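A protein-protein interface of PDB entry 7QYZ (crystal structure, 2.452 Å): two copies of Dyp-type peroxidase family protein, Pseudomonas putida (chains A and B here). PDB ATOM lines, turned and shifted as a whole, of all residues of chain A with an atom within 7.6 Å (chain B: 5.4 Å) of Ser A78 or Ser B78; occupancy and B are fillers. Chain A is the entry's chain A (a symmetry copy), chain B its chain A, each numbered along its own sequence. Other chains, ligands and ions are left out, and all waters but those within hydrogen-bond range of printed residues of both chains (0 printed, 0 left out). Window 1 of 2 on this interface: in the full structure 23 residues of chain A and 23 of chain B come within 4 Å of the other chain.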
ATOM      1  N   PRO A  66     -15.591  20.092 -14.818  1.00  0.00           N
ATOM      2  CA  PRO A  66     -16.148  21.018 -13.826  1.00  0.00           C
ATOM      3  C   PRO A  66     -16.065  22.465 -14.291  1.00  0.00           C
ATOM      4  O   PRO A  66     -15.322  22.813 -15.213  1.00  0.00           O
ATOM      5  CB  PRO A  66     -15.275  20.784 -12.587  1.00  0.00           C
ATOM      6  CG  PRO A  66     -14.702  19.424 -12.777  1.00  0.00           C
ATOM      7  CD  PRO A  66     -14.500  19.278 -14.254  1.00  0.00           C
ATOM      8  N   PHE A  67     -16.855  23.312 -13.638  1.00  0.00           N
ATOM      9  CA  PHE A  67     -16.813  24.741 -13.911  1.00  0.00           C
ATOM     10  C   PHE A  67     -15.407  25.270 -13.639  1.00  0.00           C
ATOM     11  O   PHE A  67     -14.820  24.943 -12.599  1.00  0.00           O
ATOM     12  CB  PHE A  67     -17.837  25.476 -13.046  1.00  0.00           C
ATOM     13  CG  PHE A  67     -18.000  26.930 -13.393  1.00  0.00           C
ATOM     14  CD1 PHE A  67     -17.237  27.897 -12.763  1.00  0.00           C
ATOM     15  CD2 PHE A  67     -18.921  27.328 -14.346  1.00  0.00           C
ATOM     16  CE1 PHE A  67     -17.385  29.234 -13.080  1.00  0.00           C
ATOM     17  CE2 PHE A  67     -19.074  28.664 -14.667  1.00  0.00           C
ATOM     18  CZ  PHE A  67     -18.304  29.618 -14.032  1.00  0.00           C
ATOM     19  N   PRO A  68     -14.843  26.082 -14.528  1.00  0.00           N
ATOM     20  CA  PRO A  68     -13.424  26.432 -14.412  1.00  0.00           C
ATOM     21  C   PRO A  68     -13.149  27.376 -13.253  1.00  0.00           C
ATOM     22  O   PRO A  68     -14.034  28.058 -12.730  1.00  0.00           O
ATOM     23  CB  PRO A  68     -13.120  27.104 -15.755  1.00  0.00           C
ATOM     24  CG  PRO A  68     -14.424  27.694 -16.166  1.00  0.00           C
ATOM     25  CD  PRO A  68     -15.477  26.728 -15.690  1.00  0.00           C
ATOM     26  N   LEU A  69     -11.882  27.399 -12.852  1.00  0.00           N
ATOM     27  CA  LEU A  69     -11.385  28.309 -11.829  1.00  0.00           C
ATOM     28  C   LEU A  69     -10.642  29.444 -12.519  1.00  0.00           C
ATOM     29  O   LEU A  69      -9.627  29.211 -13.186  1.00  0.00           O
ATOM     30  CB  LEU A  69     -10.472  27.576 -10.847  1.00  0.00           C
ATOM     31  CG  LEU A  69      -9.761  28.427  -9.796  1.00  0.00           C
ATOM     32  CD1 LEU A  69     -10.762  29.087  -8.860  1.00  0.00           C
ATOM     33  CD2 LEU A  69      -8.774  27.575  -9.017  1.00  0.00           C
ATOM     34  N   LEU A  70     -11.146  30.663 -12.366  1.00  0.00           N
ATOM     35  CA  LEU A  70     -10.623  31.830 -13.073  1.00  0.00           C
ATOM     36  C   LEU A  70      -9.910  32.733 -12.072  1.00  0.00           C
ATOM     37  O   LEU A  70     -10.547  33.517 -11.364  1.00  0.00           O
ATOM     38  CB  LEU A  70     -11.743  32.574 -13.795  1.00  0.00           C
ATOM     39  CG  LEU A  70     -12.017  32.167 -15.245  1.00  0.00           C
ATOM     40  CD1 LEU A  70     -12.332  30.684 -15.368  1.00  0.00           C
ATOM     41  CD2 LEU A  70     -13.151  33.000 -15.812  1.00  0.00           C
ATOM     42  N   GLU A  75     -14.853  37.629  -8.969  1.00  0.00           N
ATOM     43  CA  GLU A  75     -15.155  36.336  -8.365  1.00  0.00           C
ATOM     44  C   GLU A  75     -16.222  35.625  -9.190  1.00  0.00           C
ATOM     45  O   GLU A  75     -17.371  36.073  -9.253  1.00  0.00           O
ATOM     46  CB  GLU A  75     -15.613  36.516  -6.919  1.00  0.00           C
ATOM     47  CG  GLU A  75     -14.633  37.294  -6.051  1.00  0.00           C
ATOM     48  CD  GLU A  75     -15.185  37.586  -4.668  1.00  0.00           C
ATOM     49  OE1 GLU A  75     -16.218  36.987  -4.302  1.00  0.00           O
ATOM     50  OE2 GLU A  75     -14.590  38.417  -3.949  1.00  0.00           O
ATOM     51  N   ASN A  76     -15.838  34.519  -9.819  1.00  0.00           N
ATOM     52  CA  ASN A  76     -16.778  33.618 -10.486  1.00  0.00           C
ATOM     53  C   ASN A  76     -16.705  32.271  -9.785  1.00  0.00           C
ATOM     54  O   ASN A  76     -15.814  31.456 -10.089  1.00  0.00           O
ATOM     55  CB  ASN A  76     -16.457  33.479 -11.973  1.00  0.00           C
ATOM     56  CG  ASN A  76     -16.683  34.768 -12.739  1.00  0.00           C
ATOM     57  OD1 ASN A  76     -17.802  35.068 -13.156  1.00  0.00           O
ATOM     58  ND2 ASN A  76     -15.620  35.539 -12.929  1.00  0.00           N
ATOM     59  N   PRO A  77     -17.595  31.995  -8.834  1.00  0.00           N
ATOM     60  CA  PRO A  77     -17.469  30.772  -8.037  1.00  0.00           C
ATOM     61  C   PRO A  77     -17.712  29.526  -8.871  1.00  0.00           C
ATOM     62  O   PRO A  77     -18.441  29.545  -9.867  1.00  0.00           O
ATOM     63  CB  PRO A  77     -18.551  30.934  -6.961  1.00  0.00           C
ATOM     64  CG  PRO A  77     -18.918  32.392  -6.981  1.00  0.00           C
ATOM     65  CD  PRO A  77     -18.726  32.827  -8.396  1.00  0.00           C
ATOM     66  N   SER A  78     -17.087  28.433  -8.450  1.00  0.00           N
ATOM     67  CA  SER A  78     -17.250  27.128  -9.082  1.00  0.00           C
ATOM     68  C   SER A  78     -18.020  26.250  -8.101  1.00  0.00           C
ATOM     69  O   SER A  78     -17.439  25.638  -7.203  1.00  0.00           O
ATOM     70  CB  SER A  78     -15.900  26.519  -9.451  1.00  0.00           C
ATOM     71  OG  SER A  78     -16.061  25.336 -10.215  1.00  0.00           O
ATOM     72  N   THR A  79     -19.341  26.202  -8.274  1.00  0.00           N
ATOM     73  CA  THR A  79     -20.199  25.393  -7.417  1.00  0.00           C
ATOM     74  C   THR A  79     -20.707  24.184  -8.188  1.00  0.00           C
ATOM     75  O   THR A  79     -21.918  24.008  -8.357  1.00  0.00           O
ATOM     76  CB  THR A  79     -21.371  26.222  -6.894  1.00  0.00           C
ATOM     77  OG1 THR A  79     -20.933  27.562  -6.643  1.00  0.00           O
ATOM     78  CG2 THR A  79     -21.906  25.627  -5.600  1.00  0.00           C
ATOM     79  N   GLN A  80     -19.787  23.353  -8.668  1.00  0.00           N
ATOM     80  CA  GLN A  80     -20.161  22.226  -9.510  1.00  0.00           C
ATOM     81  C   GLN A  80     -20.928  21.186  -8.702  1.00  0.00           C
ATOM     82  O   GLN A  80     -20.502  20.791  -7.612  1.00  0.00           O
ATOM     83  CB  GLN A  80     -18.916  21.605 -10.141  1.00  0.00           C
ATOM     84  CG  GLN A  80     -19.217  20.517 -11.157  1.00  0.00           C
ATOM     85  CD  GLN A  80     -19.970  21.036 -12.368  1.00  0.00           C
ATOM     86  OE1 GLN A  80     -19.490  21.916 -13.082  1.00  0.00           O
ATOM     87  NE2 GLN A  80     -21.158  20.492 -12.603  1.00  0.00           N
ATOM     88  N   HIS A  81     -22.064  20.752  -9.232  1.00  0.00           N
ATOM     89  CA  HIS A  81     -22.886  19.719  -8.621  1.00  0.00           C
ATOM     90  C   HIS A  81     -22.958  18.511  -9.549  1.00  0.00           C
ATOM     91  O   HIS A  81     -22.423  18.515 -10.660  1.00  0.00           O
ATOM     92  CB  HIS A  81     -24.287  20.246  -8.299  1.00  0.00           C
ATOM     93  CG  HIS A  81     -24.293  21.376  -7.318  1.00  0.00           C
ATOM     94  ND1 HIS A  81     -24.677  22.653  -7.660  1.00  0.00           N
ATOM     95  CD2 HIS A  81     -23.957  21.421  -6.008  1.00  0.00           C
ATOM     96  CE1 HIS A  81     -24.580  23.438  -6.601  1.00  0.00           C
ATOM     97  NE2 HIS A  81     -24.144  22.714  -5.586  1.00  0.00           N
ATOM     98  N   GLN A 158     -25.092  30.006 -14.097  1.00  0.00           N
ATOM     99  CA  GLN A 158     -24.508  30.987 -13.194  1.00  0.00           C
ATOM    100  C   GLN A 158     -25.630  31.801 -12.570  1.00  0.00           C
ATOM    101  O   GLN A 158     -26.445  32.385 -13.291  1.00  0.00           O
ATOM    102  CB  GLN A 158     -23.532  31.903 -13.936  1.00  0.00           C
ATOM    103  CG  GLN A 158     -22.138  31.926 -13.347  1.00  0.00           C
ATOM    104  CD  GLN A 158     -21.198  32.815 -14.129  1.00  0.00           C
ATOM    105  OE1 GLN A 158     -21.493  33.208 -15.256  1.00  0.00           O
ATOM    106  NE2 GLN A 158     -20.060  33.144 -13.532  1.00  0.00           N
ATOM    107  N   LEU A 264     -23.265  33.984  -7.898  1.00  0.00           N
ATOM    108  CA  LEU A 264     -23.208  33.246  -6.644  1.00  0.00           C
ATOM    109  C   LEU A 264     -22.863  31.779  -6.832  1.00  0.00           C
ATOM    110  O   LEU A 264     -22.290  31.169  -5.925  1.00  0.00           O
ATOM    111  CB  LEU A 264     -24.544  33.356  -5.903  1.00  0.00           C
ATOM    112  CG  LEU A 264     -25.038  34.770  -5.590  1.00  0.00           C
ATOM    113  CD1 LEU A 264     -26.387  34.724  -4.887  1.00  0.00           C
ATOM    114  CD2 LEU A 264     -24.020  35.525  -4.750  1.00  0.00           C
ATOM    115  N   THR A 265     -23.205  31.196  -7.978  1.00  0.00           N
ATOM    116  CA  THR A 265     -22.912  29.803  -8.285  1.00  0.00           C
ATOM    117  C   THR A 265     -22.277  29.717  -9.669  1.00  0.00           C
ATOM    118  O   THR A 265     -22.083  30.725 -10.355  1.00  0.00           O
ATOM    119  CB  THR A 265     -24.175  28.932  -8.214  1.00  0.00           C
ATOM    120  OG1 THR A 265     -25.110  29.352  -9.215  1.00  0.00           O
ATOM    121  CG2 THR A 265     -24.827  29.031  -6.841  1.00  0.00           C
ATOM    122  N   GLY A 266     -21.956  28.494 -10.076  1.00  0.00           N
ATOM    123  CA  GLY A 266     -21.373  28.242 -11.378  1.00  0.00           C
ATOM    124  C   GLY A 266     -21.119  26.765 -11.593  1.00  0.00           C
ATOM    125  O   GLY A 266     -20.544  26.102 -10.724  1.00  0.00           O
ATOM    126  N   GLY A 267     -21.544  26.233 -12.734  1.00  0.00           N
ATOM    127  CA  GLY A 267     -21.383  24.815 -12.993  1.00  0.00           C
ATOM    128  C   GLY A 267     -21.485  24.497 -14.463  1.00  0.00           C
ATOM    129  O   GLY A 267     -22.187  25.177 -15.219  1.00  0.00           O
ATOM    130  N   TYR A 268     -20.767  23.455 -14.875  1.00  0.00           N
ATOM    131  CA  TYR A 268     -20.867  22.896 -16.214  1.00  0.00           C
ATOM    132  C   TYR A 268     -21.664  21.600 -16.162  1.00  0.00           C
ATOM    133  O   TYR A 268     -21.451  20.766 -15.276  1.00  0.00           O
ATOM    134  CB  TYR A 268     -19.486  22.619 -16.809  1.00  0.00           C
ATOM    135  CG  TYR A 268     -18.749  23.826 -17.337  1.00  0.00           C
ATOM    136  CD1 TYR A 268     -19.325  25.090 -17.314  1.00  0.00           C
ATOM    137  CD2 TYR A 268     -17.476  23.696 -17.879  1.00  0.00           C
ATOM    138  CE1 TYR A 268     -18.647  26.193 -17.806  1.00  0.00           C
ATOM    139  CE2 TYR A 268     -16.792  24.789 -18.374  1.00  0.00           C
ATOM    140  CZ  TYR A 268     -17.383  26.034 -18.338  1.00  0.00           C
ATOM    141  OH  TYR A 268     -16.698  27.121 -18.831  1.00  0.00           O
ATOM    142  N   PRO B  66      -6.009  31.118  -5.715  1.00  0.00           N
ATOM    143  CA  PRO B  66      -7.399  30.791  -5.383  1.00  0.00           C
ATOM    144  C   PRO B  66      -7.542  29.362  -4.878  1.00  0.00           C
ATOM    145  O   PRO B  66      -6.663  28.515  -5.059  1.00  0.00           O
ATOM    146  CB  PRO B  66      -8.141  30.985  -6.712  1.00  0.00           C
ATOM    147  CG  PRO B  66      -7.274  31.902  -7.500  1.00  0.00           C
ATOM    148  CD  PRO B  66      -5.869  31.554  -7.116  1.00  0.00           C
ATOM    149  N   PHE B  67      -8.672  29.107  -4.225  1.00  0.00           N
ATOM    150  CA  PHE B  67      -8.986  27.762  -3.767  1.00  0.00           C
ATOM    151  C   PHE B  67      -9.033  26.815  -4.963  1.00  0.00           C
ATOM    152  O   PHE B  67      -9.645  27.149  -5.987  1.00  0.00           O
ATOM    153  CB  PHE B  67     -10.323  27.753  -3.027  1.00  0.00           C
ATOM    154  CG  PHE B  67     -10.641  26.448  -2.353  1.00  0.00           C
ATOM    155  CD1 PHE B  67     -11.357  25.466  -3.015  1.00  0.00           C
ATOM    156  CD2 PHE B  67     -10.228  26.206  -1.054  1.00  0.00           C
ATOM    157  CE1 PHE B  67     -11.651  24.264  -2.398  1.00  0.00           C
ATOM    158  CE2 PHE B  67     -10.520  25.007  -0.431  1.00  0.00           C
ATOM    159  CZ  PHE B  67     -11.233  24.035  -1.105  1.00  0.00           C
ATOM    160  N   PRO B  68      -8.417  25.639  -4.877  1.00  0.00           N
ATOM    161  CA  PRO B  68      -8.253  24.802  -6.069  1.00  0.00           C
ATOM    162  C   PRO B  68      -9.561  24.175  -6.527  1.00  0.00           C
ATOM    163  O   PRO B  68     -10.539  24.068  -5.782  1.00  0.00           O
ATOM    164  CB  PRO B  68      -7.259  23.730  -5.609  1.00  0.00           C
ATOM    165  CG  PRO B  68      -7.505  23.617  -4.144  1.00  0.00           C
ATOM    166  CD  PRO B  68      -7.838  25.010  -3.677  1.00  0.00           C
ATOM    167  N   LEU B  69      -9.559  23.762  -7.790  1.00  0.00           N
ATOM    168  CA  LEU B  69     -10.671  23.042  -8.394  1.00  0.00           C
ATOM    169  C   LEU B  69     -10.306  21.565  -8.458  1.00  0.00           C
ATOM    170  O   LEU B  69      -9.342  21.190  -9.136  1.00  0.00           O
ATOM    171  CB  LEU B  69     -10.979  23.588  -9.788  1.00  0.00           C
ATOM    172  CG  LEU B  69     -12.031  22.843 -10.607  1.00  0.00           C
ATOM    173  CD1 LEU B  69     -13.394  22.910  -9.935  1.00  0.00           C
ATOM    174  CD2 LEU B  69     -12.093  23.410 -12.014  1.00  0.00           C
ATOM    175  N   ASN B  76     -16.148  19.888  -3.652  1.00  0.00           N
ATOM    176  CA  ASN B  76     -15.477  20.871  -2.803  1.00  0.00           C
ATOM    177  C   ASN B  76     -15.536  22.214  -3.513  1.00  0.00           C
ATOM    178  O   ASN B  76     -14.694  22.496  -4.387  1.00  0.00           O
ATOM    179  CB  ASN B  76     -14.032  20.467  -2.517  1.00  0.00           C
ATOM    180  CG  ASN B  76     -13.937  19.218  -1.661  1.00  0.00           C
ATOM    181  OD1 ASN B  76     -14.009  19.285  -0.434  1.00  0.00           O
ATOM    182  ND2 ASN B  76     -13.773  18.070  -2.306  1.00  0.00           N
ATOM    183  N   PRO B  77     -16.510  23.063  -3.196  1.00  0.00           N
ATOM    184  CA  PRO B  77     -16.687  24.303  -3.959  1.00  0.00           C
ATOM    185  C   PRO B  77     -15.535  25.269  -3.742  1.00  0.00           C
ATOM    186  O   PRO B  77     -14.880  25.273  -2.697  1.00  0.00           O
ATOM    187  CB  PRO B  77     -17.999  24.877  -3.408  1.00  0.00           C
ATOM    188  CG  PRO B  77     -18.662  23.737  -2.687  1.00  0.00           C
ATOM    189  CD  PRO B  77     -17.543  22.898  -2.163  1.00  0.00           C
ATOM    190  N   SER B  78     -15.293  26.095  -4.754  1.00  0.00           N
ATOM    191  CA  SER B  78     -14.272  27.136  -4.706  1.00  0.00           C
ATOM    192  C   SER B  78     -15.000  28.475  -4.667  1.00  0.00           C
ATOM    193  O   SER B  78     -15.378  29.024  -5.704  1.00  0.00           O
ATOM    194  CB  SER B  78     -13.325  27.038  -5.898  1.00  0.00           C
ATOM    195  OG  SER B  78     -12.236  27.935  -5.765  1.00  0.00           O
ATOM    196  N   THR B  79     -15.206  28.993  -3.456  1.00  0.00           N
ATOM    197  CA  THR B  79     -15.879  30.273  -3.272  1.00  0.00           C
ATOM    198  C   THR B  79     -14.872  31.329  -2.840  1.00  0.00           C
ATOM    199  O   THR B  79     -15.000  31.916  -1.761  1.00  0.00           O
ATOM    200  CB  THR B  79     -16.997  30.149  -2.238  1.00  0.00           C
ATOM    201  OG1 THR B  79     -17.621  28.867  -2.363  1.00  0.00           O
ATOM    202  CG2 THR B  79     -18.044  31.230  -2.456  1.00  0.00           C
ATOM    203  N   GLN B  80     -13.863  31.566  -3.672  1.00  0.00           N
ATOM    204  CA  GLN B  80     -12.788  32.477  -3.306  1.00  0.00           C
ATOM    205  C   GLN B  80     -13.301  33.911  -3.245  1.00  0.00           C
ATOM    206  O   GLN B  80     -13.975  34.382  -4.166  1.00  0.00           O
ATOM    207  CB  GLN B  80     -11.637  32.360  -4.305  1.00  0.00           C
ATOM    208  CG  GLN B  80     -10.405  33.162  -3.922  1.00  0.00           C
ATOM    209  CD  GLN B  80      -9.768  32.679  -2.633  1.00  0.00           C
ATOM    210  OE1 GLN B  80      -9.355  31.524  -2.526  1.00  0.00           O
ATOM    211  NE2 GLN B  80      -9.685  33.563  -1.646  1.00  0.00           N
ATOM    212  N   GLY B 266     -15.282  27.529   0.176  1.00  0.00           N
ATOM    213  CA  GLY B 266     -13.880  27.170   0.127  1.00  0.00           C
ATOM    214  C   GLY B 266     -13.036  28.309  -0.404  1.00  0.00           C
ATOM    215  O   GLY B 266     -13.369  28.897  -1.438  1.00  0.00           O
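CB of Pro A66 touches CD1 of Leu B69 (3.9 Å).
Leu B69 touches Phe A67 (CD2 to O, 3.2 Å).
Pro B66 touches Leu A69.
Phe B67 touches Leu A69.
Leu A69 touches Ser B78 (CD1 to OG, 3.6 Å).
Pro A77 touches Ser B78 (CA to O, 3.6 Å).
Leu B69 touches Ser A78 (CD1 to OG, 3.6 Å).
O of Ser A78 touches CA of Pro B77, at 3.6 Å.
Hydrophobic or aromatic side chains of chain A that line the printed part of chain B: Pro A66, Leu A69 and Pro A77.
Of the 10 printed residues of chain B, 6 touch a printed residue of chain A.
Hydrophobic or aromatic side chains of chain B within 4 Å of the printed part of chain A: Pro B66, Leu B69 and Pro B77.
Among the printed residues, no Asp or Glu carboxylate lies within 4 Å of a Lys or Arg side-chain nitrogen of the other chain.
The backbone carbonyl oxygen of Phe B67 lies within hydrogen-bond range of the side-chain hydroxyl of Ser B78 (2.7 Å).
The backbone NH (N) of Phe A67 sits at hydrogen-bond distance from the side-chain amide oxygen (OE1) of Gln A80 (3.0 Å).
The backbone NH of Phe B67 sits at hydrogen-bond distance from the side-chain amide oxygen of Gln B80, 3.0 Å away.
The backbone carbonyl oxygen of Phe A67 is in hydrogen-bond range of the side-chain hydroxyl of Ser A78 (2.7 Å).
Pro A66 touches Leu B69, and with the chains exchanged Leu A69 touches Pro B66.
Leu A69 touches Ser B78, and with the chains exchanged Ser A78 touches Leu B69.
Pro A77 touches Ser B78, and with the chains exchanged Ser A78 touches Pro B77.
Ser B78 touches its own counterpart, Ser A78.
10 positions are printed for both chains.
Of the 10 pairs that touch across the chains among the printed residues, 9 have their exchanged pair printed and touching as well.
The side-chain carboxylate (OE1) of Glu A75 lies close to the backbone carbonyl oxygen (O) of Gln B80.
The backbone carbonyl oxygen of Ser A78 is in hydrogen-bond range of the backbone NH of Ser B78 (3.3 Å).
Ser A78 touches three residues of chain B.
Of chain A, only Leu A69, Pro A77 and Ser A78 come within 4 Å of Ser B78.
Of the printed residues of chain A, Leu B69 touches Pro A66 (3.9 Å), Phe A67 (3.2 Å) and Ser A78 (3.6 Å).
Of the printed residues of chain A, Pro B66 touches Leu A69 (3.9 Å).
Of the printed residues of chain A, Phe B67 touches Leu A69 (3.2 Å).
Printed residues of chain B within 4 Å of Pro A66: Leu B69 (3.9 Å).
Of the printed residues of chain B, Phe A67 touches Leu B69 (3.2 Å).
Asn B76 touches none of the printed residues of chain A.
Thr A265 touches none of the printed residues of chain B.
The nearest printed residue of chain A that does not touch Leu B69 is Pro A68 (4.1 Å).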
